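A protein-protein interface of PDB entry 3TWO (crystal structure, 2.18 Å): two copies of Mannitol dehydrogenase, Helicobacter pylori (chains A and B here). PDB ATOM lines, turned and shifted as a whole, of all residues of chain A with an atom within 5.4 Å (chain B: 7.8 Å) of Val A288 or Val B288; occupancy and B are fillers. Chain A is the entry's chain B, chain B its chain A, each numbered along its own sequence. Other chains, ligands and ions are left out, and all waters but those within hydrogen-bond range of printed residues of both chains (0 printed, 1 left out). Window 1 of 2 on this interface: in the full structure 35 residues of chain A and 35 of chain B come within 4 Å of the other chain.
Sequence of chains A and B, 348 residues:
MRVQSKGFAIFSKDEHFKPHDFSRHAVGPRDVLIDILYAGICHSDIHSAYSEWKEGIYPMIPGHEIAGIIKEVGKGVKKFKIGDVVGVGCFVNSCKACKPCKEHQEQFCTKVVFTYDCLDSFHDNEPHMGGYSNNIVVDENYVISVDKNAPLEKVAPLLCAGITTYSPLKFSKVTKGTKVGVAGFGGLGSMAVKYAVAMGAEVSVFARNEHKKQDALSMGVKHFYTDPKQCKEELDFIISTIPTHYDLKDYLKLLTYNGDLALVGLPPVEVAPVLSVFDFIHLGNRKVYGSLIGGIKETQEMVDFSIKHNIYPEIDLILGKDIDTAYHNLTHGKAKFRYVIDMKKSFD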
ATOM      1  N   LEU A 252       1.851   5.540  13.776  1.00  0.00           N
ATOM      2  CA  LEU A 252       2.697   4.548  13.134  1.00  0.00           C
ATOM      3  C   LEU A 252       2.113   4.167  11.774  1.00  0.00           C
ATOM      4  O   LEU A 252       2.832   4.058  10.793  1.00  0.00           O
ATOM      5  CB  LEU A 252       2.905   3.308  14.047  1.00  0.00           C
ATOM      6  CG  LEU A 252       3.712   2.113  13.508  1.00  0.00           C
ATOM      7  CD1 LEU A 252       5.185   2.519  13.219  1.00  0.00           C
ATOM      8  CD2 LEU A 252       3.729   0.944  14.470  1.00  0.00           C
ATOM      9  N   LEU A 261       9.320   6.716  13.241  1.00  0.00           N
ATOM     10  CA  LEU A 261       8.536   7.456  14.229  1.00  0.00           C
ATOM     11  C   LEU A 261       9.438   7.631  15.450  1.00  0.00           C
ATOM     12  O   LEU A 261       9.903   6.624  16.033  1.00  0.00           O
ATOM     13  CB  LEU A 261       7.327   6.631  14.649  1.00  0.00           C
ATOM     14  CG  LEU A 261       6.459   7.024  15.855  1.00  0.00           C
ATOM     15  CD1 LEU A 261       5.941   8.488  15.676  1.00  0.00           C
ATOM     16  CD2 LEU A 261       5.255   6.087  15.972  1.00  0.00           C
ATOM     17  N   LEU A 263       9.904   9.173  19.132  1.00  0.00           N
ATOM     18  CA  LEU A 263       9.079   9.484  20.290  1.00  0.00           C
ATOM     19  C   LEU A 263       9.923  10.310  21.238  1.00  0.00           C
ATOM     20  O   LEU A 263      10.965   9.837  21.719  1.00  0.00           O
ATOM     21  CB  LEU A 263       8.634   8.188  21.004  1.00  0.00           C
ATOM     22  CG  LEU A 263       7.865   7.224  20.133  1.00  0.00           C
ATOM     23  CD1 LEU A 263       7.589   5.852  20.798  1.00  0.00           C
ATOM     24  CD2 LEU A 263       6.558   7.855  19.503  1.00  0.00           C
ATOM     25  N   LEU A 275       3.141  -0.132  22.363  1.00  0.00           N
ATOM     26  CA  LEU A 275       2.927  -0.886  21.157  1.00  0.00           C
ATOM     27  C   LEU A 275       3.286  -2.333  21.470  1.00  0.00           C
ATOM     28  O   LEU A 275       4.306  -2.586  22.080  1.00  0.00           O
ATOM     29  CB  LEU A 275       3.819  -0.319  20.032  1.00  0.00           C
ATOM     30  CG  LEU A 275       3.358   0.995  19.365  1.00  0.00           C
ATOM     31  CD1 LEU A 275       4.524   1.642  18.586  1.00  0.00           C
ATOM     32  CD2 LEU A 275       2.100   0.767  18.448  1.00  0.00           C
ATOM     33  N   PHE A 280       3.359  -3.958  15.897  1.00  0.00           N
ATOM     34  CA  PHE A 280       4.498  -3.777  14.980  1.00  0.00           C
ATOM     35  C   PHE A 280       4.374  -4.617  13.706  1.00  0.00           C
ATOM     36  O   PHE A 280       4.626  -4.122  12.617  1.00  0.00           O
ATOM     37  CB  PHE A 280       5.826  -4.084  15.639  1.00  0.00           C
ATOM     38  CG  PHE A 280       6.312  -2.987  16.536  1.00  0.00           C
ATOM     39  CD1 PHE A 280       6.208  -3.094  17.933  1.00  0.00           C
ATOM     40  CD2 PHE A 280       6.888  -1.849  16.007  1.00  0.00           C
ATOM     41  CE1 PHE A 280       6.709  -2.038  18.769  1.00  0.00           C
ATOM     42  CE2 PHE A 280       7.370  -0.811  16.852  1.00  0.00           C
ATOM     43  CZ  PHE A 280       7.277  -0.919  18.215  1.00  0.00           C
ATOM     44  N   ARG A 286       7.910  -0.312   9.536  1.00  0.00           N
ATOM     45  CA  ARG A 286       7.845   1.077   9.948  1.00  0.00           C
ATOM     46  C   ARG A 286       8.524   1.137  11.285  1.00  0.00           C
ATOM     47  O   ARG A 286       8.096   0.441  12.254  1.00  0.00           O
ATOM     48  CB  ARG A 286       6.392   1.499  10.079  1.00  0.00           C
ATOM     49  CG  ARG A 286       5.656   1.495   8.770  1.00  0.00           C
ATOM     50  CD  ARG A 286       4.192   1.597   9.079  1.00  0.00           C
ATOM     51  NE  ARG A 286       3.352   1.704   7.886  1.00  0.00           N
ATOM     52  CZ  ARG A 286       2.733   0.688   7.298  1.00  0.00           C
ATOM     53  NH1 ARG A 286       2.919  -0.550   7.716  1.00  0.00           N
ATOM     54  NH2 ARG A 286       1.975   0.893   6.237  1.00  0.00           N
ATOM     55  N   LYS A 287       9.596   1.930  11.370  1.00  0.00           N
ATOM     56  CA  LYS A 287      10.479   1.805  12.536  1.00  0.00           C
ATOM     57  C   LYS A 287      10.109   2.813  13.634  1.00  0.00           C
ATOM     58  O   LYS A 287       9.718   3.944  13.332  1.00  0.00           O
ATOM     59  CB  LYS A 287      11.924   2.027  12.070  1.00  0.00           C
ATOM     60  CG  LYS A 287      12.410   1.006  10.958  1.00  0.00           C
ATOM     61  CD  LYS A 287      13.921   1.015  10.868  1.00  0.00           C
ATOM     62  CE  LYS A 287      14.344   0.360   9.594  1.00  0.00           C
ATOM     63  NZ  LYS A 287      15.829   0.349   9.539  1.00  0.00           N
ATOM     64  N   VAL A 288      10.267   2.441  14.892  1.00  0.00           N
ATOM     65  CA  VAL A 288       9.947   3.328  16.007  1.00  0.00           C
ATOM     66  C   VAL A 288      11.215   3.439  16.890  1.00  0.00           C
ATOM     67  O   VAL A 288      11.916   2.439  17.123  1.00  0.00           O
ATOM     68  CB  VAL A 288       8.795   2.747  16.882  1.00  0.00           C
ATOM     69  CG1 VAL A 288       8.505   3.642  18.060  1.00  0.00           C
ATOM     70  CG2 VAL A 288       7.441   2.496  16.069  1.00  0.00           C
ATOM     71  N   TYR A 289      11.557   4.623  17.359  1.00  0.00           N
ATOM     72  CA  TYR A 289      12.600   4.670  18.399  1.00  0.00           C
ATOM     73  C   TYR A 289      12.268   5.813  19.313  1.00  0.00           C
ATOM     74  O   TYR A 289      11.410   6.672  18.956  1.00  0.00           O
ATOM     75  CB  TYR A 289      13.980   4.847  17.817  1.00  0.00           C
ATOM     76  CG  TYR A 289      14.131   6.121  17.005  1.00  0.00           C
ATOM     77  CD1 TYR A 289      14.587   7.288  17.632  1.00  0.00           C
ATOM     78  CD2 TYR A 289      13.837   6.164  15.606  1.00  0.00           C
ATOM     79  CE1 TYR A 289      14.790   8.508  16.921  1.00  0.00           C
ATOM     80  CE2 TYR A 289      14.023   7.416  14.870  1.00  0.00           C
ATOM     81  CZ  TYR A 289      14.486   8.555  15.546  1.00  0.00           C
ATOM     82  OH  TYR A 289      14.730   9.766  14.923  1.00  0.00           O
ATOM     83  N   GLY A 290      12.918   5.839  20.476  1.00  0.00           N
ATOM     84  CA  GLY A 290      12.772   6.971  21.395  1.00  0.00           C
ATOM     85  C   GLY A 290      14.014   7.853  21.318  1.00  0.00           C
ATOM     86  O   GLY A 290      15.067   7.400  20.873  1.00  0.00           O
ATOM     87  N   PHE B 171      15.731  -6.317   4.494  1.00  0.00           N
ATOM     88  CA  PHE B 171      15.130  -4.969   4.702  1.00  0.00           C
ATOM     89  C   PHE B 171      16.108  -4.140   5.534  1.00  0.00           C
ATOM     90  O   PHE B 171      16.270  -2.954   5.289  1.00  0.00           O
ATOM     91  CB  PHE B 171      13.788  -5.115   5.425  1.00  0.00           C
ATOM     92  CG  PHE B 171      13.209  -3.809   5.956  1.00  0.00           C
ATOM     93  CD1 PHE B 171      12.736  -2.808   5.077  1.00  0.00           C
ATOM     94  CD2 PHE B 171      13.053  -3.620   7.341  1.00  0.00           C
ATOM     95  CE1 PHE B 171      12.187  -1.639   5.601  1.00  0.00           C
ATOM     96  CE2 PHE B 171      12.486  -2.472   7.845  1.00  0.00           C
ATOM     97  CZ  PHE B 171      12.070  -1.475   6.976  1.00  0.00           C
ATOM     98  N   LEU B 248      10.547  -7.375  25.958  1.00  0.00           N
ATOM     99  CA  LEU B 248      11.233  -6.773  24.837  1.00  0.00           C
ATOM    100  C   LEU B 248      12.432  -5.916  25.208  1.00  0.00           C
ATOM    101  O   LEU B 248      13.369  -5.807  24.404  1.00  0.00           O
ATOM    102  CB  LEU B 248      10.250  -5.936  23.995  1.00  0.00           C
ATOM    103  CG  LEU B 248       9.323  -6.833  23.155  1.00  0.00           C
ATOM    104  CD1 LEU B 248       8.042  -6.124  22.811  1.00  0.00           C
ATOM    105  CD2 LEU B 248      10.053  -7.376  21.923  1.00  0.00           C
ATOM    106  N   TYR B 251      16.022  -7.293  24.926  1.00  0.00           N
ATOM    107  CA  TYR B 251      16.643  -7.342  23.593  1.00  0.00           C
ATOM    108  C   TYR B 251      16.968  -5.959  23.061  1.00  0.00           C
ATOM    109  O   TYR B 251      18.045  -5.778  22.484  1.00  0.00           O
ATOM    110  CB  TYR B 251      15.794  -8.132  22.604  1.00  0.00           C
ATOM    111  CG  TYR B 251      15.822  -9.600  22.992  1.00  0.00           C
ATOM    112  CD1 TYR B 251      14.795 -10.188  23.747  1.00  0.00           C
ATOM    113  CD2 TYR B 251      16.928 -10.372  22.671  1.00  0.00           C
ATOM    114  CE1 TYR B 251      14.890 -11.575  24.130  1.00  0.00           C
ATOM    115  CE2 TYR B 251      17.036 -11.693  23.058  1.00  0.00           C
ATOM    116  CZ  TYR B 251      16.024 -12.313  23.751  1.00  0.00           C
ATOM    117  OH  TYR B 251      16.229 -13.635  24.058  1.00  0.00           O
ATOM    118  N   LEU B 252      16.042  -5.005  23.240  1.00  0.00           N
ATOM    119  CA  LEU B 252      16.211  -3.634  22.729  1.00  0.00           C
ATOM    120  C   LEU B 252      17.513  -3.029  23.290  1.00  0.00           C
ATOM    121  O   LEU B 252      18.286  -2.391  22.576  1.00  0.00           O
ATOM    122  CB  LEU B 252      15.005  -2.755  23.077  1.00  0.00           C
ATOM    123  CG  LEU B 252      14.991  -1.262  22.564  1.00  0.00           C
ATOM    124  CD1 LEU B 252      15.096  -1.197  21.063  1.00  0.00           C
ATOM    125  CD2 LEU B 252      13.745  -0.535  22.952  1.00  0.00           C
ATOM    126  N   LEU B 255      21.038  -3.476  21.481  1.00  0.00           N
ATOM    127  CA  LEU B 255      21.319  -2.900  20.154  1.00  0.00           C
ATOM    128  C   LEU B 255      22.325  -1.773  20.302  1.00  0.00           C
ATOM    129  O   LEU B 255      22.289  -1.001  21.262  1.00  0.00           O
ATOM    130  CB  LEU B 255      20.042  -2.362  19.486  1.00  0.00           C
ATOM    131  CG  LEU B 255      19.025  -3.386  18.989  1.00  0.00           C
ATOM    132  CD1 LEU B 255      17.865  -2.648  18.336  1.00  0.00           C
ATOM    133  CD2 LEU B 255      19.734  -4.341  18.018  1.00  0.00           C
ATOM    134  N   GLY B 259      20.828   0.739  15.873  1.00  0.00           N
ATOM    135  CA  GLY B 259      20.613  -0.672  15.594  1.00  0.00           C
ATOM    136  C   GLY B 259      19.141  -0.979  15.313  1.00  0.00           C
ATOM    137  O   GLY B 259      18.257  -0.150  15.641  1.00  0.00           O
ATOM    138  N   ASP B 260      18.853  -2.161  14.754  1.00  0.00           N
ATOM    139  CA  ASP B 260      17.440  -2.574  14.477  1.00  0.00           C
ATOM    140  C   ASP B 260      17.009  -3.813  15.238  1.00  0.00           C
ATOM    141  O   ASP B 260      17.715  -4.839  15.207  1.00  0.00           O
ATOM    142  CB  ASP B 260      17.286  -2.983  13.024  1.00  0.00           C
ATOM    143  CG  ASP B 260      17.151  -1.840  12.085  1.00  0.00           C
ATOM    144  OD1 ASP B 260      17.022  -2.144  10.900  1.00  0.00           O
ATOM    145  OD2 ASP B 260      17.141  -0.666  12.469  1.00  0.00           O
ATOM    146  N   LEU B 261      15.839  -3.768  15.857  1.00  0.00           N
ATOM    147  CA  LEU B 261      15.231  -4.981  16.399  1.00  0.00           C
ATOM    148  C   LEU B 261      14.023  -5.322  15.522  1.00  0.00           C
ATOM    149  O   LEU B 261      13.086  -4.527  15.464  1.00  0.00           O
ATOM    150  CB  LEU B 261      14.799  -4.773  17.864  1.00  0.00           C
ATOM    151  CG  LEU B 261      13.869  -5.823  18.506  1.00  0.00           C
ATOM    152  CD1 LEU B 261      14.538  -7.152  18.538  1.00  0.00           C
ATOM    153  CD2 LEU B 261      13.454  -5.391  19.937  1.00  0.00           C
ATOM    154  N   ALA B 262      14.056  -6.503  14.896  1.00  0.00           N
ATOM    155  CA  ALA B 262      13.036  -6.955  13.962  1.00  0.00           C
ATOM    156  C   ALA B 262      12.159  -8.006  14.666  1.00  0.00           C
ATOM    157  O   ALA B 262      12.656  -9.027  15.093  1.00  0.00           O
ATOM    158  CB  ALA B 262      13.674  -7.532  12.732  1.00  0.00           C
ATOM    159  N   LEU B 263      10.859  -7.712  14.803  1.00  0.00           N
ATOM    160  CA  LEU B 263       9.918  -8.593  15.527  1.00  0.00           C
ATOM    161  C   LEU B 263       9.151  -9.474  14.551  1.00  0.00           C
ATOM    162  O   LEU B 263       8.486  -8.953  13.650  1.00  0.00           O
ATOM    163  CB  LEU B 263       8.942  -7.764  16.405  1.00  0.00           C
ATOM    164  CG  LEU B 263       9.611  -6.800  17.419  1.00  0.00           C
ATOM    165  CD1 LEU B 263       8.527  -6.089  18.253  1.00  0.00           C
ATOM    166  CD2 LEU B 263      10.547  -7.551  18.387  1.00  0.00           C
ATOM    167  N   LEU B 275       6.129  -2.381  24.277  1.00  0.00           N
ATOM    168  CA  LEU B 275       7.083  -1.390  24.727  1.00  0.00           C
ATOM    169  C   LEU B 275       6.333  -0.107  24.897  1.00  0.00           C
ATOM    170  O   LEU B 275       5.601   0.261  23.987  1.00  0.00           O
ATOM    171  CB  LEU B 275       8.174  -1.196  23.655  1.00  0.00           C
ATOM    172  CG  LEU B 275       9.132  -2.376  23.573  1.00  0.00           C
ATOM    173  CD1 LEU B 275       9.883  -2.422  22.297  1.00  0.00           C
ATOM    174  CD2 LEU B 275      10.094  -2.318  24.791  1.00  0.00           C
ATOM    175  N   SER B 276       6.496   0.588  26.024  1.00  0.00           N
ATOM    176  CA  SER B 276       5.853   1.875  26.177  1.00  0.00           C
ATOM    177  C   SER B 276       6.751   3.002  25.625  1.00  0.00           C
ATOM    178  O   SER B 276       7.962   2.810  25.368  1.00  0.00           O
ATOM    179  CB  SER B 276       5.549   2.152  27.656  1.00  0.00           C
ATOM    180  OG  SER B 276       6.756   2.519  28.306  1.00  0.00           O
ATOM    181  N   VAL B 277       6.185   4.202  25.497  1.00  0.00           N
ATOM    182  CA  VAL B 277       7.006   5.364  25.132  1.00  0.00           C
ATOM    183  C   VAL B 277       8.220   5.550  26.064  1.00  0.00           C
ATOM    184  O   VAL B 277       9.290   5.932  25.604  1.00  0.00           O
ATOM    185  CB  VAL B 277       6.177   6.658  25.032  1.00  0.00           C
ATOM    186  CG1 VAL B 277       5.183   6.522  23.905  1.00  0.00           C
ATOM    187  CG2 VAL B 277       5.413   6.903  26.265  1.00  0.00           C
ATOM    188  N   PHE B 280      11.063   3.188  25.015  1.00  0.00           N
ATOM    189  CA  PHE B 280      11.799   3.607  23.862  1.00  0.00           C
ATOM    190  C   PHE B 280      12.768   4.731  24.198  1.00  0.00           C
ATOM    191  O   PHE B 280      13.881   4.747  23.682  1.00  0.00           O
ATOM    192  CB  PHE B 280      10.886   4.077  22.761  1.00  0.00           C
ATOM    193  CG  PHE B 280      10.250   2.968  21.964  1.00  0.00           C
ATOM    194  CD1 PHE B 280       8.899   2.688  22.120  1.00  0.00           C
ATOM    195  CD2 PHE B 280      10.993   2.274  21.008  1.00  0.00           C
ATOM    196  CE1 PHE B 280       8.292   1.674  21.376  1.00  0.00           C
ATOM    197  CE2 PHE B 280      10.410   1.274  20.239  1.00  0.00           C
ATOM    198  CZ  PHE B 280       9.056   0.958  20.443  1.00  0.00           C
ATOM    199  N   LEU B 283      15.697   3.746  26.357  1.00  0.00           N
ATOM    200  CA  LEU B 283      16.621   3.008  25.516  1.00  0.00           C
ATOM    201  C   LEU B 283      16.713   3.677  24.149  1.00  0.00           C
ATOM    202  O   LEU B 283      16.436   3.065  23.145  1.00  0.00           O
ATOM    203  CB  LEU B 283      16.173   1.528  25.393  1.00  0.00           C
ATOM    204  CG  LEU B 283      16.136   0.732  26.730  1.00  0.00           C
ATOM    205  CD1 LEU B 283      15.492  -0.686  26.585  1.00  0.00           C
ATOM    206  CD2 LEU B 283      17.551   0.682  27.375  1.00  0.00           C
ATOM    207  N   ASN B 285      17.461   5.791  20.541  1.00  0.00           N
ATOM    208  CA  ASN B 285      18.264   5.619  19.293  1.00  0.00           C
ATOM    209  C   ASN B 285      18.408   4.180  18.807  1.00  0.00           C
ATOM    210  O   ASN B 285      19.389   3.851  18.121  1.00  0.00           O
ATOM    211  CB  ASN B 285      19.663   6.310  19.428  1.00  0.00           C
ATOM    212  CG  ASN B 285      19.515   7.786  19.596  1.00  0.00           C
ATOM    213  OD1 ASN B 285      19.157   8.523  18.654  1.00  0.00           O
ATOM    214  ND2 ASN B 285      19.729   8.238  20.772  1.00  0.00           N
ATOM    215  N   ARG B 286      17.450   3.331  19.168  1.00  0.00           N
ATOM    216  CA  ARG B 286      17.490   1.934  18.784  1.00  0.00           C
ATOM    217  C   ARG B 286      16.111   1.643  18.199  1.00  0.00           C
ATOM    218  O   ARG B 286      15.066   1.854  18.854  1.00  0.00           O
ATOM    219  CB  ARG B 286      17.741   1.088  20.005  1.00  0.00           C
ATOM    220  CG  ARG B 286      19.068   1.502  20.743  1.00  0.00           C
ATOM    221  CD  ARG B 286      19.099   0.734  22.073  1.00  0.00           C
ATOM    222  NE  ARG B 286      20.339   0.781  22.816  1.00  0.00           N
ATOM    223  CZ  ARG B 286      20.576   1.639  23.831  1.00  0.00           C
ATOM    224  NH1 ARG B 286      19.683   2.587  24.149  1.00  0.00           N
ATOM    225  NH2 ARG B 286      21.724   1.581  24.526  1.00  0.00           N
ATOM    226  N   LYS B 287      16.089   1.218  16.956  1.00  0.00           N
ATOM    227  CA  LYS B 287      14.839   1.187  16.222  1.00  0.00           C
ATOM    228  C   LYS B 287      14.223  -0.184  16.314  1.00  0.00           C
ATOM    229  O   LYS B 287      14.928  -1.209  16.306  1.00  0.00           O
ATOM    230  CB  LYS B 287      15.065   1.548  14.760  1.00  0.00           C
ATOM    231  CG  LYS B 287      15.791   2.863  14.559  1.00  0.00           C
ATOM    232  CD  LYS B 287      15.757   3.357  13.095  1.00  0.00           C
ATOM    233  CE  LYS B 287      16.606   4.610  12.932  1.00  0.00           C
ATOM    234  NZ  LYS B 287      16.402   5.219  11.601  1.00  0.00           N
ATOM    235  N   VAL B 288      12.892  -0.202  16.399  1.00  0.00           N
ATOM    236  CA  VAL B 288      12.096  -1.452  16.430  1.00  0.00           C
ATOM    237  C   VAL B 288      11.099  -1.419  15.274  1.00  0.00           C
ATOM    238  O   VAL B 288      10.495  -0.344  14.996  1.00  0.00           O
ATOM    239  CB  VAL B 288      11.339  -1.581  17.783  1.00  0.00           C
ATOM    240  CG1 VAL B 288      10.466  -2.864  17.850  1.00  0.00           C
ATOM    241  CG2 VAL B 288      12.373  -1.568  18.962  1.00  0.00           C
ATOM    242  N   TYR B 289      10.924  -2.562  14.595  1.00  0.00           N
ATOM    243  CA  TYR B 289       9.817  -2.718  13.618  1.00  0.00           C
ATOM    244  C   TYR B 289       9.386  -4.175  13.601  1.00  0.00           C
ATOM    245  O   TYR B 289      10.165  -5.060  14.049  1.00  0.00           O
ATOM    246  CB  TYR B 289      10.262  -2.306  12.213  1.00  0.00           C
ATOM    247  CG  TYR B 289      11.335  -3.214  11.597  1.00  0.00           C
ATOM    248  CD1 TYR B 289      10.977  -4.304  10.784  1.00  0.00           C
ATOM    249  CD2 TYR B 289      12.711  -2.947  11.790  1.00  0.00           C
ATOM    250  CE1 TYR B 289      11.927  -5.111  10.199  1.00  0.00           C
ATOM    251  CE2 TYR B 289      13.664  -3.745  11.235  1.00  0.00           C
ATOM    252  CZ  TYR B 289      13.284  -4.831  10.426  1.00  0.00           C
ATOM    253  OH  TYR B 289      14.240  -5.627   9.850  1.00  0.00           O
ATOM    254  N   GLY B 290       8.171  -4.418  13.088  1.00  0.00           N
ATOM    255  CA  GLY B 290       7.648  -5.807  12.864  1.00  0.00           C
ATOM    256  C   GLY B 290       7.766  -6.199  11.388  1.00  0.00           C
ATOM    257  O   GLY B 290       7.856  -5.332  10.522  1.00  0.00           O
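The backbone carbonyl oxygen (O) of Leu A275 sits at hydrogen-bond distance from the backbone NH (N) of Leu B275 (2.9 Å). The backbone NH (N) of Asn B285 lies within hydrogen-bond range of the backbone carbonyl oxygen (O) of Gly A290, 2.9 Å away. The backbone carbonyl oxygen (O) of Val B288 sits at hydrogen-bond distance from the backbone NH (N) of Val A288 (2.8 Å). The side-chain carboxylate (OD1) of Asp B260 is in salt-bridge range of the side-chain amino group (NZ) of Lys A287, at 3.1 Å.
Hydrophobic or aromatic side chains of chain A within 4 Å of the printed part of chain B: Leu A263, Phe A280, Val A288 and Tyr A289. Printed residues of chain B that touch a printed residue of chain A: Phe B171, Asp B260, Leu B263, Leu B275, Val B277, Phe B280, Asn B285, Arg B286, Lys B287, Val B288, Tyr B289 and Gly B290. Hydrophobic or aromatic side chains of chain B that line the printed part of chain A: Phe B171, Leu B263, Val B277, Phe B280, Val B288 and Tyr B289. Along chain B the printed residues that touch a printed residue of chain A span positions 171 to 290. Among the printed residues, 23 pairs touch across the chains.
The backbone carbonyl oxygen of Tyr B289 lies within hydrogen-bond range of the backbone NH of Leu B263 (2.8 Å). O of Leu B283 sits close to NH1 of Arg B286. N of Leu B261 sits at hydrogen-bond distance from O of Lys B287. The backbone NH of Leu A261 is in hydrogen-bond range of the backbone carbonyl oxygen of Lys A287. The backbone NH of Leu A263 sits at hydrogen-bond distance from the backbone carbonyl oxygen of Tyr A289 (2.9 Å). The backbone NH (N) of Tyr B289 is in hydrogen-bond range of the backbone carbonyl oxygen (O) of Leu B261, 3.0 Å away.
Among the printed residues, merely in contact across the chains: Lys A287 with Val B288 (3.3 Å), Val A288 with Lys B287 (3.3 Å), Tyr A289 with Arg B286 (3.3 Å), Gly A290 with Phe B280 (3.4 Å), Phe A280 with Phe B280 (3.4 Å), Phe A280 with Gly B290 (3.5 Å), Arg A286 with Tyr B289 (3.5 Å), Val A288 with Phe B280 (3.6 Å), Val A288 with Arg B286 (3.6 Å), Phe A280 with Val B288 (3.7 Å), Leu A263 with Phe B280 (3.7 Å), Lys A287 with Lys B287 (3.7 Å), Arg A286 with Val B288 (3.7 Å), Phe A280 with Leu B263 (3.8 Å), Lys A287 with Phe B171 (3.8 Å), Phe A280 with Tyr B289 (3.9 Å), Tyr A289 with Phe B280 (3.9 Å), Tyr A289 with Lys B287 (3.98 Å) and Leu A263 with Val B277 (3.99 Å).
Phe A280 touches Val B288, and with the chains exchanged Val A288 touches Phe B280. Arg A286 touches Val B288, and with the chains exchanged Val A288 touches Arg B286. Arg A286 touches Tyr B289, and with the chains exchanged Tyr A289 touches Arg B286. Val A288 touches its own counterpart, Val B288. Positions printed for both chains: 252, 261, 263, 275, 280, 286, 287, 288, 289 and 290. Of the 23 pairs that touch across the chains among the printed residues, 18 have their exchanged pair printed and touching as well.
Val A288 touches just these residues of chain B: Phe B280 (3.6 Å), Arg B286 (3.6 Å), Lys B287 (3.3 Å) and Val B288 (2.8 Å). Val B288 touches just these residues of chain A: Phe A280, Arg A286, Lys A287 and Val A288. Of the printed residues of chain A, Val B277 touches Leu A263 (3.99 Å). Printed residues of chain A within 4 Å of Tyr B289: Phe A280 (3.9 Å) and Arg A286 (3.5 Å). Printed residues of chain A within 4 Å of Leu B263: Phe A280. Of the printed residues of chain B, Arg A286 touches Val B288 and Tyr B289. Of the printed residues of chain A, Arg B286 touches Val A288 (3.6 Å) and Tyr A289 (3.3 Å). The nearest residue of chain B that does not touch Val A288 is Tyr B289 (5.1 Å). The nearest residue of chain A that does not touch Val B288 is Tyr A289 (5.1 Å).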
